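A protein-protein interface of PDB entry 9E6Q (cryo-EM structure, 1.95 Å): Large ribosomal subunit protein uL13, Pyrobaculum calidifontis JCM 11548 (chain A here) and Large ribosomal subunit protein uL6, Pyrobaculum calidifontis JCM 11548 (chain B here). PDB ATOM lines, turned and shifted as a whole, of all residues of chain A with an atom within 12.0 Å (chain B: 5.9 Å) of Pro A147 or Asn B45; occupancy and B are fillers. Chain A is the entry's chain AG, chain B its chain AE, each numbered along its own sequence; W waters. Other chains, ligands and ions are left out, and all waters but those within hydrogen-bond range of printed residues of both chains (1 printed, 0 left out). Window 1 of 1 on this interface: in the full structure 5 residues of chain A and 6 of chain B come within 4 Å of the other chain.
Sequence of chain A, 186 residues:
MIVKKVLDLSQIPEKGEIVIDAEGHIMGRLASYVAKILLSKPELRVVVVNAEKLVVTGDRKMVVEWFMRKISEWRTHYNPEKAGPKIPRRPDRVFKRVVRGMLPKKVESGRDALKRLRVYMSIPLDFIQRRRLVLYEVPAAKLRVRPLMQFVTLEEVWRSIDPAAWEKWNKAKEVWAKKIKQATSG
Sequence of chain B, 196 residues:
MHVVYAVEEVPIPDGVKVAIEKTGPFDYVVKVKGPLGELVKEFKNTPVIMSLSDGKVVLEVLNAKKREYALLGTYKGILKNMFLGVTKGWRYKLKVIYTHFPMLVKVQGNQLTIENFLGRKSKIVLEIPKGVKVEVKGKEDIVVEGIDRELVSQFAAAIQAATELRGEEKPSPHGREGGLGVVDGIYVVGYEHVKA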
ATOM      1  N   VAL A  55      -9.087  32.205  22.705  1.00  0.00           N
ATOM      2  CA  VAL A  55      -9.943  32.344  21.540  1.00  0.00           C
ATOM      3  C   VAL A  55      -9.890  33.780  21.045  1.00  0.00           C
ATOM      4  O   VAL A  55      -9.941  34.723  21.839  1.00  0.00           O
ATOM      5  CB  VAL A  55     -11.379  31.916  21.890  1.00  0.00           C
ATOM      6  CG1 VAL A  55     -12.365  32.505  20.922  1.00  0.00           C
ATOM      7  CG2 VAL A  55     -11.472  30.408  21.889  1.00  0.00           C
ATOM      8  N   VAL A  56      -9.772  33.943  19.732  1.00  0.00           N
ATOM      9  CA  VAL A  56      -9.927  35.235  19.073  1.00  0.00           C
ATOM     10  C   VAL A  56     -11.146  35.138  18.168  1.00  0.00           C
ATOM     11  O   VAL A  56     -11.187  34.297  17.263  1.00  0.00           O
ATOM     12  CB  VAL A  56      -8.674  35.629  18.273  1.00  0.00           C
ATOM     13  CG1 VAL A  56      -8.849  36.995  17.641  1.00  0.00           C
ATOM     14  CG2 VAL A  56      -7.460  35.614  19.155  1.00  0.00           C
ATOM     15  N   THR A  57     -12.139  35.982  18.417  1.00  0.00           N
ATOM     16  CA  THR A  57     -13.354  35.953  17.620  1.00  0.00           C
ATOM     17  C   THR A  57     -13.092  36.514  16.230  1.00  0.00           C
ATOM     18  O   THR A  57     -12.200  37.336  16.023  1.00  0.00           O
ATOM     19  CB  THR A  57     -14.471  36.753  18.289  1.00  0.00           C
ATOM     20  OG1 THR A  57     -14.070  38.121  18.413  1.00  0.00           O
ATOM     21  CG2 THR A  57     -14.790  36.193  19.655  1.00  0.00           C
ATOM     22  N   GLY A  58     -13.878  36.057  15.272  1.00  0.00           N
ATOM     23  CA  GLY A  58     -13.774  36.518  13.905  1.00  0.00           C
ATOM     24  C   GLY A  58     -13.418  35.394  12.950  1.00  0.00           C
ATOM     25  O   GLY A  58     -13.061  34.287  13.339  1.00  0.00           O
ATOM     26  N   ASP A  59     -13.526  35.724  11.672  1.00  0.00           N
ATOM     27  CA  ASP A  59     -13.256  34.763  10.614  1.00  0.00           C
ATOM     28  C   ASP A  59     -11.795  34.333  10.637  1.00  0.00           C
ATOM     29  O   ASP A  59     -10.898  35.150  10.845  1.00  0.00           O
ATOM     30  CB  ASP A  59     -13.611  35.385   9.270  1.00  0.00           C
ATOM     31  CG  ASP A  59     -13.507  34.411   8.134  1.00  0.00           C
ATOM     32  OD1 ASP A  59     -14.019  33.282   8.266  1.00  0.00           O
ATOM     33  OD2 ASP A  59     -12.901  34.774   7.108  1.00  0.00           O
ATOM     34  N   ARG A  60     -11.556  33.036  10.416  1.00  0.00           N
ATOM     35  CA  ARG A  60     -10.201  32.501  10.517  1.00  0.00           C
ATOM     36  C   ARG A  60      -9.260  33.177   9.535  1.00  0.00           C
ATOM     37  O   ARG A  60      -8.148  33.570   9.899  1.00  0.00           O
ATOM     38  CB  ARG A  60     -10.197  30.994  10.280  1.00  0.00           C
ATOM     39  CG  ARG A  60      -8.841  30.357  10.530  1.00  0.00           C
ATOM     40  CD  ARG A  60      -8.570  29.185   9.625  1.00  0.00           C
ATOM     41  NE  ARG A  60      -7.140  28.928   9.514  1.00  0.00           N
ATOM     42  CZ  ARG A  60      -6.441  29.088   8.400  1.00  0.00           C
ATOM     43  NH1 ARG A  60      -7.013  29.486   7.277  1.00  0.00           N
ATOM     44  NH2 ARG A  60      -5.133  28.857   8.419  1.00  0.00           N
ATOM     45  N   LEU A 143     -15.843  32.910  26.349  1.00  0.00           N
ATOM     46  CA  LEU A 143     -16.583  32.968  25.099  1.00  0.00           C
ATOM     47  C   LEU A 143     -17.936  32.293  25.265  1.00  0.00           C
ATOM     48  O   LEU A 143     -18.019  31.143  25.697  1.00  0.00           O
ATOM     49  CB  LEU A 143     -15.794  32.297  23.979  1.00  0.00           C
ATOM     50  CG  LEU A 143     -16.536  32.014  22.673  1.00  0.00           C
ATOM     51  CD1 LEU A 143     -16.614  33.255  21.815  1.00  0.00           C
ATOM     52  CD2 LEU A 143     -15.861  30.898  21.918  1.00  0.00           C
ATOM     53  N   ARG A 144     -18.993  33.016  24.922  1.00  0.00           N
ATOM     54  CA  ARG A 144     -20.339  32.461  24.888  1.00  0.00           C
ATOM     55  C   ARG A 144     -20.545  31.836  23.517  1.00  0.00           C
ATOM     56  O   ARG A 144     -20.675  32.547  22.520  1.00  0.00           O
ATOM     57  CB  ARG A 144     -21.371  33.546  25.165  1.00  0.00           C
ATOM     58  CG  ARG A 144     -22.765  33.040  25.447  1.00  0.00           C
ATOM     59  CD  ARG A 144     -23.620  34.088  26.158  1.00  0.00           C
ATOM     60  NE  ARG A 144     -23.871  35.274  25.345  1.00  0.00           N
ATOM     61  CZ  ARG A 144     -23.114  36.365  25.330  1.00  0.00           C
ATOM     62  NH1 ARG A 144     -22.060  36.491  26.122  1.00  0.00           N
ATOM     63  NH2 ARG A 144     -23.427  37.359  24.505  1.00  0.00           N
ATOM     64  N   VAL A 145     -20.564  30.514  23.466  1.00  0.00           N
ATOM     65  CA  VAL A 145     -20.577  29.806  22.193  1.00  0.00           C
ATOM     66  C   VAL A 145     -21.978  29.857  21.602  1.00  0.00           C
ATOM     67  O   VAL A 145     -22.961  29.492  22.256  1.00  0.00           O
ATOM     68  CB  VAL A 145     -20.093  28.359  22.371  1.00  0.00           C
ATOM     69  CG1 VAL A 145     -20.603  27.490  21.249  1.00  0.00           C
ATOM     70  CG2 VAL A 145     -18.581  28.316  22.426  1.00  0.00           C
ATOM     71  N   ARG A 146     -22.067  30.312  20.362  1.00  0.00           N
ATOM     72  CA  ARG A 146     -23.313  30.422  19.630  1.00  0.00           C
ATOM     73  C   ARG A 146     -23.149  29.786  18.261  1.00  0.00           C
ATOM     74  O   ARG A 146     -22.045  29.771  17.712  1.00  0.00           O
ATOM     75  CB  ARG A 146     -23.724  31.889  19.474  1.00  0.00           C
ATOM     76  CG  ARG A 146     -24.621  32.382  20.575  1.00  0.00           C
ATOM     77  CD  ARG A 146     -24.370  33.837  20.881  1.00  0.00           C
ATOM     78  NE  ARG A 146     -22.977  34.097  21.213  1.00  0.00           N
ATOM     79  CZ  ARG A 146     -22.454  35.309  21.329  1.00  0.00           C
ATOM     80  NH1 ARG A 146     -23.177  36.394  21.113  1.00  0.00           N
ATOM     81  NH2 ARG A 146     -21.177  35.434  21.674  1.00  0.00           N
ATOM     82  N   PRO A 147     -24.225  29.251  17.688  1.00  0.00           N
ATOM     83  CA  PRO A 147     -24.127  28.671  16.347  1.00  0.00           C
ATOM     84  C   PRO A 147     -23.756  29.722  15.319  1.00  0.00           C
ATOM     85  O   PRO A 147     -24.086  30.901  15.457  1.00  0.00           O
ATOM     86  CB  PRO A 147     -25.530  28.116  16.086  1.00  0.00           C
ATOM     87  CG  PRO A 147     -26.383  28.594  17.173  1.00  0.00           C
ATOM     88  CD  PRO A 147     -25.561  29.099  18.280  1.00  0.00           C
ATOM     89  N   LEU A 148     -23.045  29.282  14.287  1.00  0.00           N
ATOM     90  CA  LEU A 148     -22.625  30.100  13.153  1.00  0.00           C
ATOM     91  C   LEU A 148     -21.727  31.262  13.558  1.00  0.00           C
ATOM     92  O   LEU A 148     -21.595  32.225  12.802  1.00  0.00           O
ATOM     93  CB  LEU A 148     -23.829  30.626  12.360  1.00  0.00           C
ATOM     94  CG  LEU A 148     -24.827  29.585  11.856  1.00  0.00           C
ATOM     95  CD1 LEU A 148     -25.829  30.208  10.904  1.00  0.00           C
ATOM     96  CD2 LEU A 148     -24.105  28.444  11.186  1.00  0.00           C
ATOM     97  N   MET A 149     -21.116  31.205  14.731  1.00  0.00           N
ATOM     98  CA  MET A 149     -20.138  32.201  15.130  1.00  0.00           C
ATOM     99  C   MET A 149     -18.741  31.721  14.769  1.00  0.00           C
ATOM    100  O   MET A 149     -18.416  30.541  14.904  1.00  0.00           O
ATOM    101  CB  MET A 149     -20.234  32.481  16.629  1.00  0.00           C
ATOM    102  CG  MET A 149     -19.899  33.904  17.020  1.00  0.00           C
ATOM    103  SD  MET A 149     -19.856  34.129  18.809  1.00  0.00           S
ATOM    104  CE  MET A 149     -18.574  35.367  18.974  1.00  0.00           C
ATOM    105  N   GLN A 150     -17.917  32.650  14.300  1.00  0.00           N
ATOM    106  CA  GLN A 150     -16.567  32.354  13.847  1.00  0.00           C
ATOM    107  C   GLN A 150     -15.556  32.774  14.901  1.00  0.00           C
ATOM    108  O   GLN A 150     -15.644  33.872  15.454  1.00  0.00           O
ATOM    109  CB  GLN A 150     -16.258  33.072  12.534  1.00  0.00           C
ATOM    110  CG  GLN A 150     -17.251  32.817  11.434  1.00  0.00           C
ATOM    111  CD  GLN A 150     -17.180  31.403  10.923  1.00  0.00           C
ATOM    112  OE1 GLN A 150     -18.007  30.563  11.267  1.00  0.00           O
ATOM    113  NE2 GLN A 150     -16.185  31.128  10.093  1.00  0.00           N
ATOM    114  N   PHE A 151     -14.599  31.894  15.174  1.00  0.00           N
ATOM    115  CA  PHE A 151     -13.484  32.208  16.053  1.00  0.00           C
ATOM    116  C   PHE A 151     -12.368  31.209  15.796  1.00  0.00           C
ATOM    117  O   PHE A 151     -12.571  30.165  15.176  1.00  0.00           O
ATOM    118  CB  PHE A 151     -13.904  32.206  17.527  1.00  0.00           C
ATOM    119  CG  PHE A 151     -14.311  30.859  18.044  1.00  0.00           C
ATOM    120  CD1 PHE A 151     -13.381  29.997  18.588  1.00  0.00           C
ATOM    121  CD2 PHE A 151     -15.631  30.464  18.001  1.00  0.00           C
ATOM    122  CE1 PHE A 151     -13.759  28.766  19.061  1.00  0.00           C
ATOM    123  CE2 PHE A 151     -16.009  29.239  18.478  1.00  0.00           C
ATOM    124  CZ  PHE A 151     -15.074  28.389  19.010  1.00  0.00           C
ATOM    125  N   VAL A 152     -11.177  31.546  16.286  1.00  0.00           N
ATOM    126  CA  VAL A 152     -10.014  30.675  16.208  1.00  0.00           C
ATOM    127  C   VAL A 152      -9.314  30.664  17.555  1.00  0.00           C
ATOM    128  O   VAL A 152      -9.529  31.533  18.400  1.00  0.00           O
ATOM    129  CB  VAL A 152      -9.029  31.102  15.101  1.00  0.00           C
ATOM    130  CG1 VAL A 152      -9.600  30.751  13.777  1.00  0.00           C
ATOM    131  CG2 VAL A 152      -8.744  32.579  15.167  1.00  0.00           C
ATOM    132  N   THR A 153      -8.474  29.659  17.754  1.00  0.00           N
ATOM    133  CA  THR A 153      -7.628  29.589  18.932  1.00  0.00           C
ATOM    134  C   THR A 153      -6.235  30.101  18.601  1.00  0.00           C
ATOM    135  O   THR A 153      -5.813  30.100  17.444  1.00  0.00           O
ATOM    136  CB  THR A 153      -7.536  28.166  19.477  1.00  0.00           C
ATOM    137  OG1 THR A 153      -6.871  27.333  18.525  1.00  0.00           O
ATOM    138  CG2 THR A 153      -8.913  27.620  19.744  1.00  0.00           C
ATOM    139  N   PHE B  26     -22.711  22.763  19.749  1.00  0.00           N
ATOM    140  CA  PHE B  26     -23.541  22.814  18.549  1.00  0.00           C
ATOM    141  C   PHE B  26     -22.938  21.978  17.430  1.00  0.00           C
ATOM    142  O   PHE B  26     -23.024  22.331  16.254  1.00  0.00           O
ATOM    143  CB  PHE B  26     -23.747  24.251  18.081  1.00  0.00           C
ATOM    144  CG  PHE B  26     -24.356  25.140  19.116  1.00  0.00           C
ATOM    145  CD1 PHE B  26     -25.713  25.117  19.349  1.00  0.00           C
ATOM    146  CD2 PHE B  26     -23.574  26.000  19.855  1.00  0.00           C
ATOM    147  CE1 PHE B  26     -26.274  25.930  20.304  1.00  0.00           C
ATOM    148  CE2 PHE B  26     -24.132  26.809  20.806  1.00  0.00           C
ATOM    149  CZ  PHE B  26     -25.482  26.777  21.031  1.00  0.00           C
ATOM    150  N   ASP B  27     -22.314  20.858  17.773  1.00  0.00           N
ATOM    151  CA  ASP B  27     -21.727  19.957  16.796  1.00  0.00           C
ATOM    152  C   ASP B  27     -22.405  18.600  16.870  1.00  0.00           C
ATOM    153  O   ASP B  27     -22.757  18.131  17.953  1.00  0.00           O
ATOM    154  CB  ASP B  27     -20.224  19.799  17.014  1.00  0.00           C
ATOM    155  CG  ASP B  27     -19.526  21.120  17.221  1.00  0.00           C
ATOM    156  OD1 ASP B  27     -18.950  21.327  18.308  1.00  0.00           O
ATOM    157  OD2 ASP B  27     -19.541  21.951  16.292  1.00  0.00           O
ATOM    158  N   TYR B  28     -22.584  17.977  15.715  1.00  0.00           N
ATOM    159  CA  TYR B  28     -23.243  16.687  15.611  1.00  0.00           C
ATOM    160  C   TYR B  28     -22.417  15.768  14.729  1.00  0.00           C
ATOM    161  O   TYR B  28     -21.774  16.212  13.776  1.00  0.00           O
ATOM    162  CB  TYR B  28     -24.640  16.817  15.016  1.00  0.00           C
ATOM    163  CG  TYR B  28     -25.684  17.306  15.976  1.00  0.00           C
ATOM    164  CD1 TYR B  28     -26.254  16.454  16.906  1.00  0.00           C
ATOM    165  CD2 TYR B  28     -26.105  18.623  15.951  1.00  0.00           C
ATOM    166  CE1 TYR B  28     -27.211  16.900  17.780  1.00  0.00           C
ATOM    167  CE2 TYR B  28     -27.058  19.078  16.821  1.00  0.00           C
ATOM    168  CZ  TYR B  28     -27.609  18.215  17.732  1.00  0.00           C
ATOM    169  OH  TYR B  28     -28.564  18.672  18.602  1.00  0.00           O
ATOM    170  N   PHE B  43     -21.842  17.684  11.330  1.00  0.00           N
ATOM    171  CA  PHE B  43     -22.553  18.956  11.233  1.00  0.00           C
ATOM    172  C   PHE B  43     -22.050  19.830  12.376  1.00  0.00           C
ATOM    173  O   PHE B  43     -22.532  19.719  13.505  1.00  0.00           O
ATOM    174  CB  PHE B  43     -24.060  18.752  11.305  1.00  0.00           C
ATOM    175  CG  PHE B  43     -24.611  17.877  10.217  1.00  0.00           C
ATOM    176  CD1 PHE B  43     -24.969  18.412   8.998  1.00  0.00           C
ATOM    177  CD2 PHE B  43     -24.772  16.523  10.417  1.00  0.00           C
ATOM    178  CE1 PHE B  43     -25.478  17.614   8.003  1.00  0.00           C
ATOM    179  CE2 PHE B  43     -25.283  15.720   9.422  1.00  0.00           C
ATOM    180  CZ  PHE B  43     -25.636  16.264   8.218  1.00  0.00           C
ATOM    181  N   LYS B  44     -21.089  20.697  12.090  1.00  0.00           N
ATOM    182  CA  LYS B  44     -20.397  21.459  13.116  1.00  0.00           C
ATOM    183  C   LYS B  44     -20.954  22.872  13.213  1.00  0.00           C
ATOM    184  O   LYS B  44     -21.341  23.476  12.212  1.00  0.00           O
ATOM    185  CB  LYS B  44     -18.900  21.525  12.821  1.00  0.00           C
ATOM    186  CG  LYS B  44     -18.185  20.186  12.869  1.00  0.00           C
ATOM    187  CD  LYS B  44     -17.022  20.150  11.887  1.00  0.00           C
ATOM    188  CE  LYS B  44     -17.329  20.963  10.634  1.00  0.00           C
ATOM    189  NZ  LYS B  44     -16.108  21.305   9.857  1.00  0.00           N
ATOM    190  N   ASN B  45     -20.985  23.393  14.439  1.00  0.00           N
ATOM    191  CA  ASN B  45     -21.333  24.791  14.694  1.00  0.00           C
ATOM    192  C   ASN B  45     -22.717  25.131  14.145  1.00  0.00           C
ATOM    193  O   ASN B  45     -22.942  26.216  13.611  1.00  0.00           O
ATOM    194  CB  ASN B  45     -20.269  25.717  14.108  1.00  0.00           C
ATOM    195  CG  ASN B  45     -20.258  27.073  14.750  1.00  0.00           C
ATOM    196  OD1 ASN B  45     -20.768  27.257  15.853  1.00  0.00           O
ATOM    197  ND2 ASN B  45     -19.678  28.042  14.060  1.00  0.00           N
ATOM    198  N   THR B  46     -23.653  24.206  14.288  1.00  0.00           N
ATOM    199  CA  THR B  46     -24.908  24.330  13.574  1.00  0.00           C
ATOM    200  C   THR B  46     -26.055  24.724  14.499  1.00  0.00           C
ATOM    201  O   THR B  46     -26.097  24.318  15.662  1.00  0.00           O
ATOM    202  CB  THR B  46     -25.260  23.016  12.864  1.00  0.00           C
ATOM    203  OG1 THR B  46     -26.481  23.175  12.139  1.00  0.00           O
ATOM    204  CG2 THR B  46     -25.409  21.877  13.852  1.00  0.00           C
ATOM    205  N   PRO B  47     -27.004  25.523  14.006  1.00  0.00           N
ATOM    206  CA  PRO B  47     -28.175  25.866  14.816  1.00  0.00           C
ATOM    207  C   PRO B  47     -29.303  24.859  14.722  1.00  0.00           C
ATOM    208  O   PRO B  47     -30.282  24.990  15.463  1.00  0.00           O
ATOM    209  CB  PRO B  47     -28.604  27.210  14.236  1.00  0.00           C
ATOM    210  CG  PRO B  47     -28.222  27.113  12.808  1.00  0.00           C
ATOM    211  CD  PRO B  47     -26.999  26.244  12.724  1.00  0.00           C
ATOM    212  N   GLU B  68     -30.555  30.745   9.390  1.00  0.00           N
ATOM    213  CA  GLU B  68     -30.657  29.499  10.137  1.00  0.00           C
ATOM    214  C   GLU B  68     -31.777  28.625   9.604  1.00  0.00           C
ATOM    215  O   GLU B  68     -31.659  27.397   9.586  1.00  0.00           O
ATOM    216  CB  GLU B  68     -30.872  29.795  11.616  1.00  0.00           C
ATOM    217  CG  GLU B  68     -29.676  30.419  12.293  1.00  0.00           C
ATOM    218  CD  GLU B  68     -29.623  31.920  12.130  1.00  0.00           C
ATOM    219  OE1 GLU B  68     -30.087  32.427  11.088  1.00  0.00           O
ATOM    220  OE2 GLU B  68     -29.108  32.599  13.042  1.00  0.00           O
HETATM  221  O   HOH W   1     -17.098  27.298  12.121  1.00  0.00           O
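O of Arg A146 lies close to OD1 of Asn B45 (3.4 Å). O of Asn B45 is in hydrogen-bond range of N of Leu A148 (3.1 Å). The backbone carbonyl oxygen (O) of Met A149 sits at hydrogen-bond distance from the side-chain amide nitrogen (ND2) of Asn B45, at 2.9 Å.
The side-chain carboxylate of Asp B27 lies within hydrogen-bond range of the backbone NH of Asn B45 (2.8 Å). O of Phe B26 sits at hydrogen-bond distance from N of Thr B46 (2.8 Å). The backbone carbonyl oxygen (O) of Arg A144 sits at hydrogen-bond distance from the guanidinium group (NH2) of Arg A146, 3.0 Å away. The guanidinium group of Arg A146 is in hydrogen-bond range of the side-chain sulfur of Met A149 (3.4 Å). O of Phe B26 lies within hydrogen-bond range of N of Asn B45 (2.9 Å).
Among the printed residues, merely in contact across the chains: Val A145 with Phe B26 (3.3 Å), Pro A147 with Phe B26 (3.6 Å), Pro A147 with Pro B47 (3.6 Å), Pro A147 with Asn B45 (3.7 Å), Pro A147 with Thr B46 (3.8 Å), Arg A146 with Phe B26 (3.9 Å) and Leu A148 with Pro B47 (3.9 Å).
Arg A60 touches none of the printed residues of chain B. Of the printed residues of chain B, Val A145 touches Phe B26 (3.3 Å). Of the printed residues of chain B, Arg A146 touches Phe B26 and Asn B45. Pro A147 touches just these residues of chain B: Phe B26 (3.6 Å), Asn B45 (3.7 Å), Thr B46 (3.8 Å) and Pro B47 (3.6 Å). Of the printed residues of chain B, Met A149 touches Asn B45 (2.9 Å). Val A152 touches none of the printed residues of chain B. Of chain A, only Val A145, Arg A146 and Pro A147 come within 4 Å of Phe B26. No residue of chain A comes within 4 Å of Asp B27. No residue of chain A comes within 4 Å of Lys B44. Asn B45 touches just these residues of chain A: Arg A146, Pro A147, Leu A148 and Met A149. The nearest residue of chain A that does not touch Asn B45 is Gln A150 (4.1 Å). The nearest printed residue of chain B that does not touch Met A149 is Thr B46 (7.5 Å).
Of the 17 printed residues of chain A, 5 touch a printed residue of chain B. Hydrophobic or aromatic side chains of chain A within 4 Å of the printed part of chain B: Val A145, Pro A147 and Leu A148. Along chain A the printed residues that touch a printed residue of chain B span positions 145 to 149. Of the 9 printed residues of chain B, 4 touch a printed residue of chain A. Among the printed residues, no Asp or Glu carboxylate lies within 4 Å of a Lys or Arg side-chain nitrogen of the other chain.
Water W1 lies within hydrogen-bond range of ND2 of Asn B45 (3.3 Å) and OE1 of Gln A150 (3.5 Å).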
